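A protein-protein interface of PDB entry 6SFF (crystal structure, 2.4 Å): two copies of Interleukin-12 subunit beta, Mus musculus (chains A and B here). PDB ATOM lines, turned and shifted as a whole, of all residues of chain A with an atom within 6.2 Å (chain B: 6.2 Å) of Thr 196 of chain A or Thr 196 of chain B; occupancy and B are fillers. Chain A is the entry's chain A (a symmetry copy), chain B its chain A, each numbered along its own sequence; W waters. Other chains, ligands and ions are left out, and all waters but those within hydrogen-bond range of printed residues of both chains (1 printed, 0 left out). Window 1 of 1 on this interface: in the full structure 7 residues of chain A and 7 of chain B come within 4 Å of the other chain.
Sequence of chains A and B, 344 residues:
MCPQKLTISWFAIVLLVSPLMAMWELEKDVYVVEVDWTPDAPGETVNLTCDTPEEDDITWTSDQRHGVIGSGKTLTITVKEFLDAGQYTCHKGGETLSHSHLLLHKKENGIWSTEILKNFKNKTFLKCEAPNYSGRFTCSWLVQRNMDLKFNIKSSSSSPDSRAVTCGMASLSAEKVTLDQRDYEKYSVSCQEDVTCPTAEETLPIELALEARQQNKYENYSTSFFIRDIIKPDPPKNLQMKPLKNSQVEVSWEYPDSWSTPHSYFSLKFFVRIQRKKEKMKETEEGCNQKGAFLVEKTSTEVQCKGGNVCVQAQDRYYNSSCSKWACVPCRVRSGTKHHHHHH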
ATOM      1  N   TYR A 133      -3.817  -4.871  -5.059  1.00  0.00           N
ATOM      2  CA  TYR A 133      -5.229  -4.595  -5.290  1.00  0.00           C
ATOM      3  C   TYR A 133      -5.726  -3.404  -4.477  1.00  0.00           C
ATOM      4  O   TYR A 133      -6.933  -3.272  -4.253  1.00  0.00           O
ATOM      5  CB  TYR A 133      -6.068  -5.833  -4.971  1.00  0.00           C
ATOM      6  CG  TYR A 133      -5.764  -7.026  -5.849  1.00  0.00           C
ATOM      7  CD1 TYR A 133      -6.435  -7.218  -7.049  1.00  0.00           C
ATOM      8  CD2 TYR A 133      -4.805  -7.960  -5.477  1.00  0.00           C
ATOM      9  CE1 TYR A 133      -6.160  -8.307  -7.856  1.00  0.00           C
ATOM     10  CE2 TYR A 133      -4.522  -9.052  -6.280  1.00  0.00           C
ATOM     11  CZ  TYR A 133      -5.202  -9.220  -7.467  1.00  0.00           C
ATOM     12  OH  TYR A 133      -4.927 -10.305  -8.266  1.00  0.00           O
ATOM     13  N   SER A 134      -4.818  -2.530  -4.039  1.00  0.00           N
ATOM     14  CA  SER A 134      -5.202  -1.385  -3.223  1.00  0.00           C
ATOM     15  C   SER A 134      -6.166  -0.449  -3.936  1.00  0.00           C
ATOM     16  O   SER A 134      -6.835   0.354  -3.275  1.00  0.00           O
ATOM     17  CB  SER A 134      -3.959  -0.593  -2.823  1.00  0.00           C
ATOM     18  OG  SER A 134      -3.392   0.051  -3.956  1.00  0.00           O
ATOM     19  N   GLY A 135      -6.250  -0.525  -5.260  1.00  0.00           N
ATOM     20  CA  GLY A 135      -6.892   0.502  -6.046  1.00  0.00           C
ATOM     21  C   GLY A 135      -5.948   1.571  -6.547  1.00  0.00           C
ATOM     22  O   GLY A 135      -6.348   2.389  -7.386  1.00  0.00           O
ATOM     23  N   ARG A 136      -4.713   1.592  -6.052  1.00  0.00           N
ATOM     24  CA  ARG A 136      -3.689   2.489  -6.562  1.00  0.00           C
ATOM     25  C   ARG A 136      -3.020   1.865  -7.781  1.00  0.00           C
ATOM     26  O   ARG A 136      -2.810   0.651  -7.841  1.00  0.00           O
ATOM     27  CB  ARG A 136      -2.655   2.777  -5.471  1.00  0.00           C
ATOM     28  CG  ARG A 136      -1.375   3.446  -5.951  1.00  0.00           C
ATOM     29  CD  ARG A 136      -1.276   4.887  -5.457  1.00  0.00           C
ATOM     30  NE  ARG A 136      -1.157   4.977  -4.003  1.00  0.00           N
ATOM     31  N   GLN A 192      -5.584   6.700  -7.794  1.00  0.00           N
ATOM     32  CA  GLN A 192      -6.172   5.869  -6.753  1.00  0.00           C
ATOM     33  C   GLN A 192      -7.672   5.797  -6.980  1.00  0.00           C
ATOM     34  O   GLN A 192      -8.333   6.833  -7.089  1.00  0.00           O
ATOM     35  CB  GLN A 192      -5.864   6.441  -5.362  1.00  0.00           C
ATOM     36  CG  GLN A 192      -6.628   5.790  -4.217  1.00  0.00           C
ATOM     37  CD  GLN A 192      -6.012   4.480  -3.769  1.00  0.00           C
ATOM     38  OE1 GLN A 192      -4.828   4.415  -3.433  1.00  0.00           O
ATOM     39  NE2 GLN A 192      -6.816   3.424  -3.758  1.00  0.00           N
ATOM     40  N   GLU A 193      -8.202   4.579  -7.062  1.00  0.00           N
ATOM     41  CA  GLU A 193      -9.647   4.401  -7.072  1.00  0.00           C
ATOM     42  C   GLU A 193     -10.223   4.904  -5.753  1.00  0.00           C
ATOM     43  O   GLU A 193      -9.767   4.513  -4.675  1.00  0.00           O
ATOM     44  CB  GLU A 193     -10.004   2.932  -7.288  1.00  0.00           C
ATOM     45  CG  GLU A 193     -11.499   2.679  -7.418  1.00  0.00           C
ATOM     46  CD  GLU A 193     -11.809   1.314  -7.997  1.00  0.00           C
ATOM     47  OE1 GLU A 193     -10.926   0.429  -7.943  1.00  0.00           O
ATOM     48  OE2 GLU A 193     -12.933   1.126  -8.506  1.00  0.00           O
ATOM     49  N   ASP A 194     -11.222   5.782  -5.843  1.00  0.00           N
ATOM     50  CA  ASP A 194     -11.702   6.479  -4.652  1.00  0.00           C
ATOM     51  C   ASP A 194     -12.278   5.503  -3.631  1.00  0.00           C
ATOM     52  O   ASP A 194     -11.962   5.579  -2.437  1.00  0.00           O
ATOM     53  CB  ASP A 194     -12.735   7.533  -5.050  1.00  0.00           C
ATOM     54  CG  ASP A 194     -12.135   8.643  -5.897  1.00  0.00           C
ATOM     55  OD1 ASP A 194     -10.924   8.918  -5.748  1.00  0.00           O
ATOM     56  OD2 ASP A 194     -12.868   9.236  -6.714  1.00  0.00           O
ATOM     57  N   VAL A 195     -13.126   4.580  -4.079  1.00  0.00           N
ATOM     58  CA  VAL A 195     -13.702   3.547  -3.222  1.00  0.00           C
ATOM     59  C   VAL A 195     -13.417   2.197  -3.865  1.00  0.00           C
ATOM     60  O   VAL A 195     -13.842   1.943  -4.999  1.00  0.00           O
ATOM     61  CB  VAL A 195     -15.211   3.744  -3.009  1.00  0.00           C
ATOM     62  CG1 VAL A 195     -15.794   2.586  -2.212  1.00  0.00           C
ATOM     63  CG2 VAL A 195     -15.473   5.070  -2.305  1.00  0.00           C
ATOM     64  N   THR A 196     -12.718   1.331  -3.139  1.00  0.00           N
ATOM     65  CA  THR A 196     -12.164   0.104  -3.688  1.00  0.00           C
ATOM     66  C   THR A 196     -12.852  -1.125  -3.108  1.00  0.00           C
ATOM     67  O   THR A 196     -13.487  -1.075  -2.052  1.00  0.00           O
ATOM     68  CB  THR A 196     -10.661   0.024  -3.403  1.00  0.00           C
ATOM     69  OG1 THR A 196     -10.455  -0.354  -2.035  1.00  0.00           O
ATOM     70  CG2 THR A 196      -9.994   1.370  -3.654  1.00  0.00           C
ATOM     71  N   CYS A 197     -12.710  -2.240  -3.822  1.00  0.00           N
ATOM     72  CA  CYS A 197     -13.167  -3.549  -3.353  1.00  0.00           C
ATOM     73  C   CYS A 197     -12.140  -4.591  -3.766  1.00  0.00           C
ATOM     74  O   CYS A 197     -12.295  -5.275  -4.784  1.00  0.00           O
ATOM     75  CB  CYS A 197     -14.550  -3.892  -3.908  1.00  0.00           C
ATOM     76  SG  CYS A 197     -15.142  -5.511  -3.356  1.00  0.00           S
ATOM     77  N   PRO A 198     -11.066  -4.743  -2.988  1.00  0.00           N
ATOM     78  CA  PRO A 198      -9.986  -5.654  -3.407  1.00  0.00           C
ATOM     79  C   PRO A 198     -10.417  -7.100  -3.587  1.00  0.00           C
ATOM     80  O   PRO A 198      -9.790  -7.824  -4.371  1.00  0.00           O
ATOM     81  CB  PRO A 198      -8.957  -5.522  -2.273  1.00  0.00           C
ATOM     82  CG  PRO A 198      -9.220  -4.176  -1.665  1.00  0.00           C
ATOM     83  CD  PRO A 198     -10.699  -3.937  -1.809  1.00  0.00           C
ATOM     84  N   THR A 199     -11.462  -7.551  -2.896  1.00  0.00           N
ATOM     85  CA  THR A 199     -11.786  -8.973  -2.885  1.00  0.00           C
ATOM     86  C   THR A 199     -12.756  -9.377  -3.990  1.00  0.00           C
ATOM     87  O   THR A 199     -12.564 -10.417  -4.629  1.00  0.00           O
ATOM     88  CB  THR A 199     -12.377  -9.371  -1.527  1.00  0.00           C
ATOM     89  OG1 THR A 199     -13.317  -8.377  -1.097  1.00  0.00           O
ATOM     90  CG2 THR A 199     -11.277  -9.514  -0.482  1.00  0.00           C
ATOM     91  N   TYR B 133     -20.313   2.417   5.845  1.00  0.00           N
ATOM     92  CA  TYR B 133     -19.881   1.158   5.252  1.00  0.00           C
ATOM     93  C   TYR B 133     -18.365   0.989   5.296  1.00  0.00           C
ATOM     94  O   TYR B 133     -17.811   0.202   4.523  1.00  0.00           O
ATOM     95  CB  TYR B 133     -20.376   1.057   3.808  1.00  0.00           C
ATOM     96  CG  TYR B 133     -21.882   1.045   3.674  1.00  0.00           C
ATOM     97  CD1 TYR B 133     -22.591  -0.148   3.710  1.00  0.00           C
ATOM     98  CD2 TYR B 133     -22.594   2.226   3.510  1.00  0.00           C
ATOM     99  CE1 TYR B 133     -23.969  -0.165   3.590  1.00  0.00           C
ATOM    100  CE2 TYR B 133     -23.973   2.219   3.389  1.00  0.00           C
ATOM    101  CZ  TYR B 133     -24.654   1.020   3.430  1.00  0.00           C
ATOM    102  OH  TYR B 133     -26.024   1.007   3.306  1.00  0.00           O
ATOM    103  N   SER B 134     -17.687   1.706   6.194  1.00  0.00           N
ATOM    104  CA  SER B 134     -16.234   1.634   6.279  1.00  0.00           C
ATOM    105  C   SER B 134     -15.731   0.235   6.603  1.00  0.00           C
ATOM    106  O   SER B 134     -14.551  -0.056   6.373  1.00  0.00           O
ATOM    107  CB  SER B 134     -15.729   2.596   7.352  1.00  0.00           C
ATOM    108  OG  SER B 134     -16.105   2.142   8.645  1.00  0.00           O
ATOM    109  N   GLY B 135     -16.586  -0.631   7.136  1.00  0.00           N
ATOM    110  CA  GLY B 135     -16.145  -1.861   7.753  1.00  0.00           C
ATOM    111  C   GLY B 135     -15.915  -1.751   9.243  1.00  0.00           C
ATOM    112  O   GLY B 135     -15.726  -2.781   9.904  1.00  0.00           O
ATOM    113  N   ARG B 136     -15.918  -0.537   9.786  1.00  0.00           N
ATOM    114  CA  ARG B 136     -15.843  -0.330  11.222  1.00  0.00           C
ATOM    115  C   ARG B 136     -17.235  -0.432  11.831  1.00  0.00           C
ATOM    116  O   ARG B 136     -18.225   0.000  11.234  1.00  0.00           O
ATOM    117  CB  ARG B 136     -15.225   1.038  11.523  1.00  0.00           C
ATOM    118  CG  ARG B 136     -15.366   1.512  12.962  1.00  0.00           C
ATOM    119  CD  ARG B 136     -14.021   1.520  13.683  1.00  0.00           C
ATOM    120  NE  ARG B 136     -13.085   2.489  13.119  1.00  0.00           N
ATOM    121  N   GLN B 192     -12.996  -3.587  13.255  1.00  0.00           N
ATOM    122  CA  GLN B 192     -12.809  -3.158  11.877  1.00  0.00           C
ATOM    123  C   GLN B 192     -12.607  -4.388  11.010  1.00  0.00           C
ATOM    124  O   GLN B 192     -11.736  -5.213  11.297  1.00  0.00           O
ATOM    125  CB  GLN B 192     -11.605  -2.213  11.760  1.00  0.00           C
ATOM    126  CG  GLN B 192     -11.174  -1.897  10.334  1.00  0.00           C
ATOM    127  CD  GLN B 192     -12.027  -0.823   9.687  1.00  0.00           C
ATOM    128  OE1 GLN B 192     -12.178   0.277  10.221  1.00  0.00           O
ATOM    129  NE2 GLN B 192     -12.588  -1.137   8.526  1.00  0.00           N
ATOM    130  N   GLU B 193     -13.419  -4.516   9.962  1.00  0.00           N
ATOM    131  CA  GLU B 193     -13.176  -5.544   8.960  1.00  0.00           C
ATOM    132  C   GLU B 193     -11.834  -5.278   8.286  1.00  0.00           C
ATOM    133  O   GLU B 193     -11.574  -4.169   7.811  1.00  0.00           O
ATOM    134  CB  GLU B 193     -14.301  -5.562   7.928  1.00  0.00           C
ATOM    135  CG  GLU B 193     -14.174  -6.681   6.905  1.00  0.00           C
ATOM    136  CD  GLU B 193     -15.460  -6.917   6.140  1.00  0.00           C
ATOM    137  OE1 GLU B 193     -16.313  -6.002   6.110  1.00  0.00           O
ATOM    138  OE2 GLU B 193     -15.618  -8.016   5.569  1.00  0.00           O
ATOM    139  N   ASP B 194     -10.978  -6.299   8.256  1.00  0.00           N
ATOM    140  CA  ASP B 194      -9.597  -6.093   7.823  1.00  0.00           C
ATOM    141  C   ASP B 194      -9.533  -5.631   6.371  1.00  0.00           C
ATOM    142  O   ASP B 194      -8.820  -4.675   6.044  1.00  0.00           O
ATOM    143  CB  ASP B 194      -8.793  -7.377   8.028  1.00  0.00           C
ATOM    144  CG  ASP B 194      -8.657  -7.748   9.496  1.00  0.00           C
ATOM    145  OD1 ASP B 194      -8.681  -6.833  10.347  1.00  0.00           O
ATOM    146  OD2 ASP B 194      -8.532  -8.953   9.800  1.00  0.00           O
ATOM    147  N   VAL B 195     -10.270  -6.297   5.484  1.00  0.00           N
ATOM    148  CA  VAL B 195     -10.350  -5.922   4.075  1.00  0.00           C
ATOM    149  C   VAL B 195     -11.821  -5.763   3.718  1.00  0.00           C
ATOM    150  O   VAL B 195     -12.599  -6.717   3.839  1.00  0.00           O
ATOM    151  CB  VAL B 195      -9.674  -6.956   3.160  1.00  0.00           C
ATOM    152  CG1 VAL B 195      -9.881  -6.590   1.697  1.00  0.00           C
ATOM    153  CG2 VAL B 195      -8.189  -7.054   3.486  1.00  0.00           C
ATOM    154  N   THR B 196     -12.195  -4.570   3.267  1.00  0.00           N
ATOM    155  CA  THR B 196     -13.587  -4.185   3.109  1.00  0.00           C
ATOM    156  C   THR B 196     -13.954  -4.014   1.641  1.00  0.00           C
ATOM    157  O   THR B 196     -13.094  -3.839   0.773  1.00  0.00           O
ATOM    158  CB  THR B 196     -13.866  -2.877   3.856  1.00  0.00           C
ATOM    159  OG1 THR B 196     -13.351  -1.775   3.094  1.00  0.00           O
ATOM    160  CG2 THR B 196     -13.203  -2.889   5.227  1.00  0.00           C
ATOM    161  N   CYS B 197     -15.258  -4.065   1.375  1.00  0.00           N
ATOM    162  CA  CYS B 197     -15.813  -3.771   0.053  1.00  0.00           C
ATOM    163  C   CYS B 197     -17.110  -2.999   0.239  1.00  0.00           C
ATOM    164  O   CYS B 197     -18.207  -3.571   0.204  1.00  0.00           O
ATOM    165  CB  CYS B 197     -16.047  -5.050  -0.753  1.00  0.00           C
ATOM    166  SG  CYS B 197     -16.744  -4.724  -2.391  1.00  0.00           S
ATOM    167  N   PRO B 198     -17.023  -1.683   0.440  1.00  0.00           N
ATOM    168  CA  PRO B 198     -18.241  -0.910   0.742  1.00  0.00           C
ATOM    169  C   PRO B 198     -19.307  -0.966  -0.339  1.00  0.00           C
ATOM    170  O   PRO B 198     -20.493  -0.803  -0.025  1.00  0.00           O
ATOM    171  CB  PRO B 198     -17.711   0.521   0.922  1.00  0.00           C
ATOM    172  CG  PRO B 198     -16.270   0.357   1.306  1.00  0.00           C
ATOM    173  CD  PRO B 198     -15.793  -0.887   0.606  1.00  0.00           C
ATOM    174  N   THR B 199     -18.936  -1.191  -1.598  1.00  0.00           N
ATOM    175  CA  THR B 199     -19.894  -1.056  -2.689  1.00  0.00           C
ATOM    176  C   THR B 199     -20.622  -2.356  -3.014  1.00  0.00           C
ATOM    177  O   THR B 199     -21.838  -2.342  -3.237  1.00  0.00           O
ATOM    178  CB  THR B 199     -19.190  -0.544  -3.951  1.00  0.00           C
ATOM    179  OG1 THR B 199     -17.942  -1.228  -4.121  1.00  0.00           O
ATOM    180  CG2 THR B 199     -18.938   0.956  -3.857  1.00  0.00           C
HETATM  181  O   HOH W   1     -11.995  -1.157   0.452  1.00  0.00           O
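SG of Cys 197 of chain A is disulfide-bonded to SG of Cys 197 of chain B (2.0 Å).
Glu 193 of chain A touches none of the printed residues of chain B. Of the printed residues of chain B, Thr 196 of chain A touches Thr 196 (3.97 Å) and Pro 198 (3.5 Å). Printed residues of chain B within 4 Å of Cys 197 of chain A: Cys 197. Gly 135 of chain B touches none of the printed residues of chain A. Of the printed residues of chain A, Cys 197 of chain B touches Cys 197. Printed residues of chain A within 4 Å of Pro 198 of chain B: Thr 196 (3.5 Å). Of the printed residues of chain A, Thr 199 of chain B touches Val 195 (3.9 Å).
Water W1 bridges O of Thr 196 of chain A (2.9 Å) and O of Thr 196 of chain B (2.9 Å).
Printed residues of chain A that touch a printed residue of chain B: Val 195, Thr 196, Cys 197, Pro 198 and Thr 199. Hydrophobic or aromatic side chains of chain A that line the printed part of chain B: Val 195 and Pro 198. Along chain A the printed residues that touch a printed residue of chain B span positions 195 to 199. Hydrophobic or aromatic side chains of chain B within 4 Å of the printed part of chain A: Val 195 and Pro 198. Among the printed residues, no Asp or Glu carboxylate lies within 4 Å of a Lys or Arg side-chain nitrogen of the other chain.
Among the printed residues, pairs that only touch across the chains: Val 195 of chain A with Thr 199 of chain B (3.9 Å), Thr 196 of chain A with Thr 196 of chain B (3.97 Å), Thr 196 of chain A with Pro 198 of chain B (3.5 Å), Pro 198 of chain A with Thr 196 of chain B (3.5 Å) and Thr 199 of chain A with Val 195 of chain B (3.9 Å).
Val 195 of chain A touches Thr 199 of chain B, and with the chains exchanged Thr 199 of chain A touches Val 195 of chain B. Thr 196 of chain B touches its own counterpart, Thr 196 of chain A. Thr 196 of chain A touches Pro 198 of chain B, and with the chains exchanged Pro 198 of chain A touches Thr 196 of chain B. Cys 197 of chain A touches its own counterpart, Cys 197 of chain B. 12 positions are printed for both chains. Of the 6 pairs that touch across the chains among the printed residues, 6 have their exchanged pair printed and touching as well.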
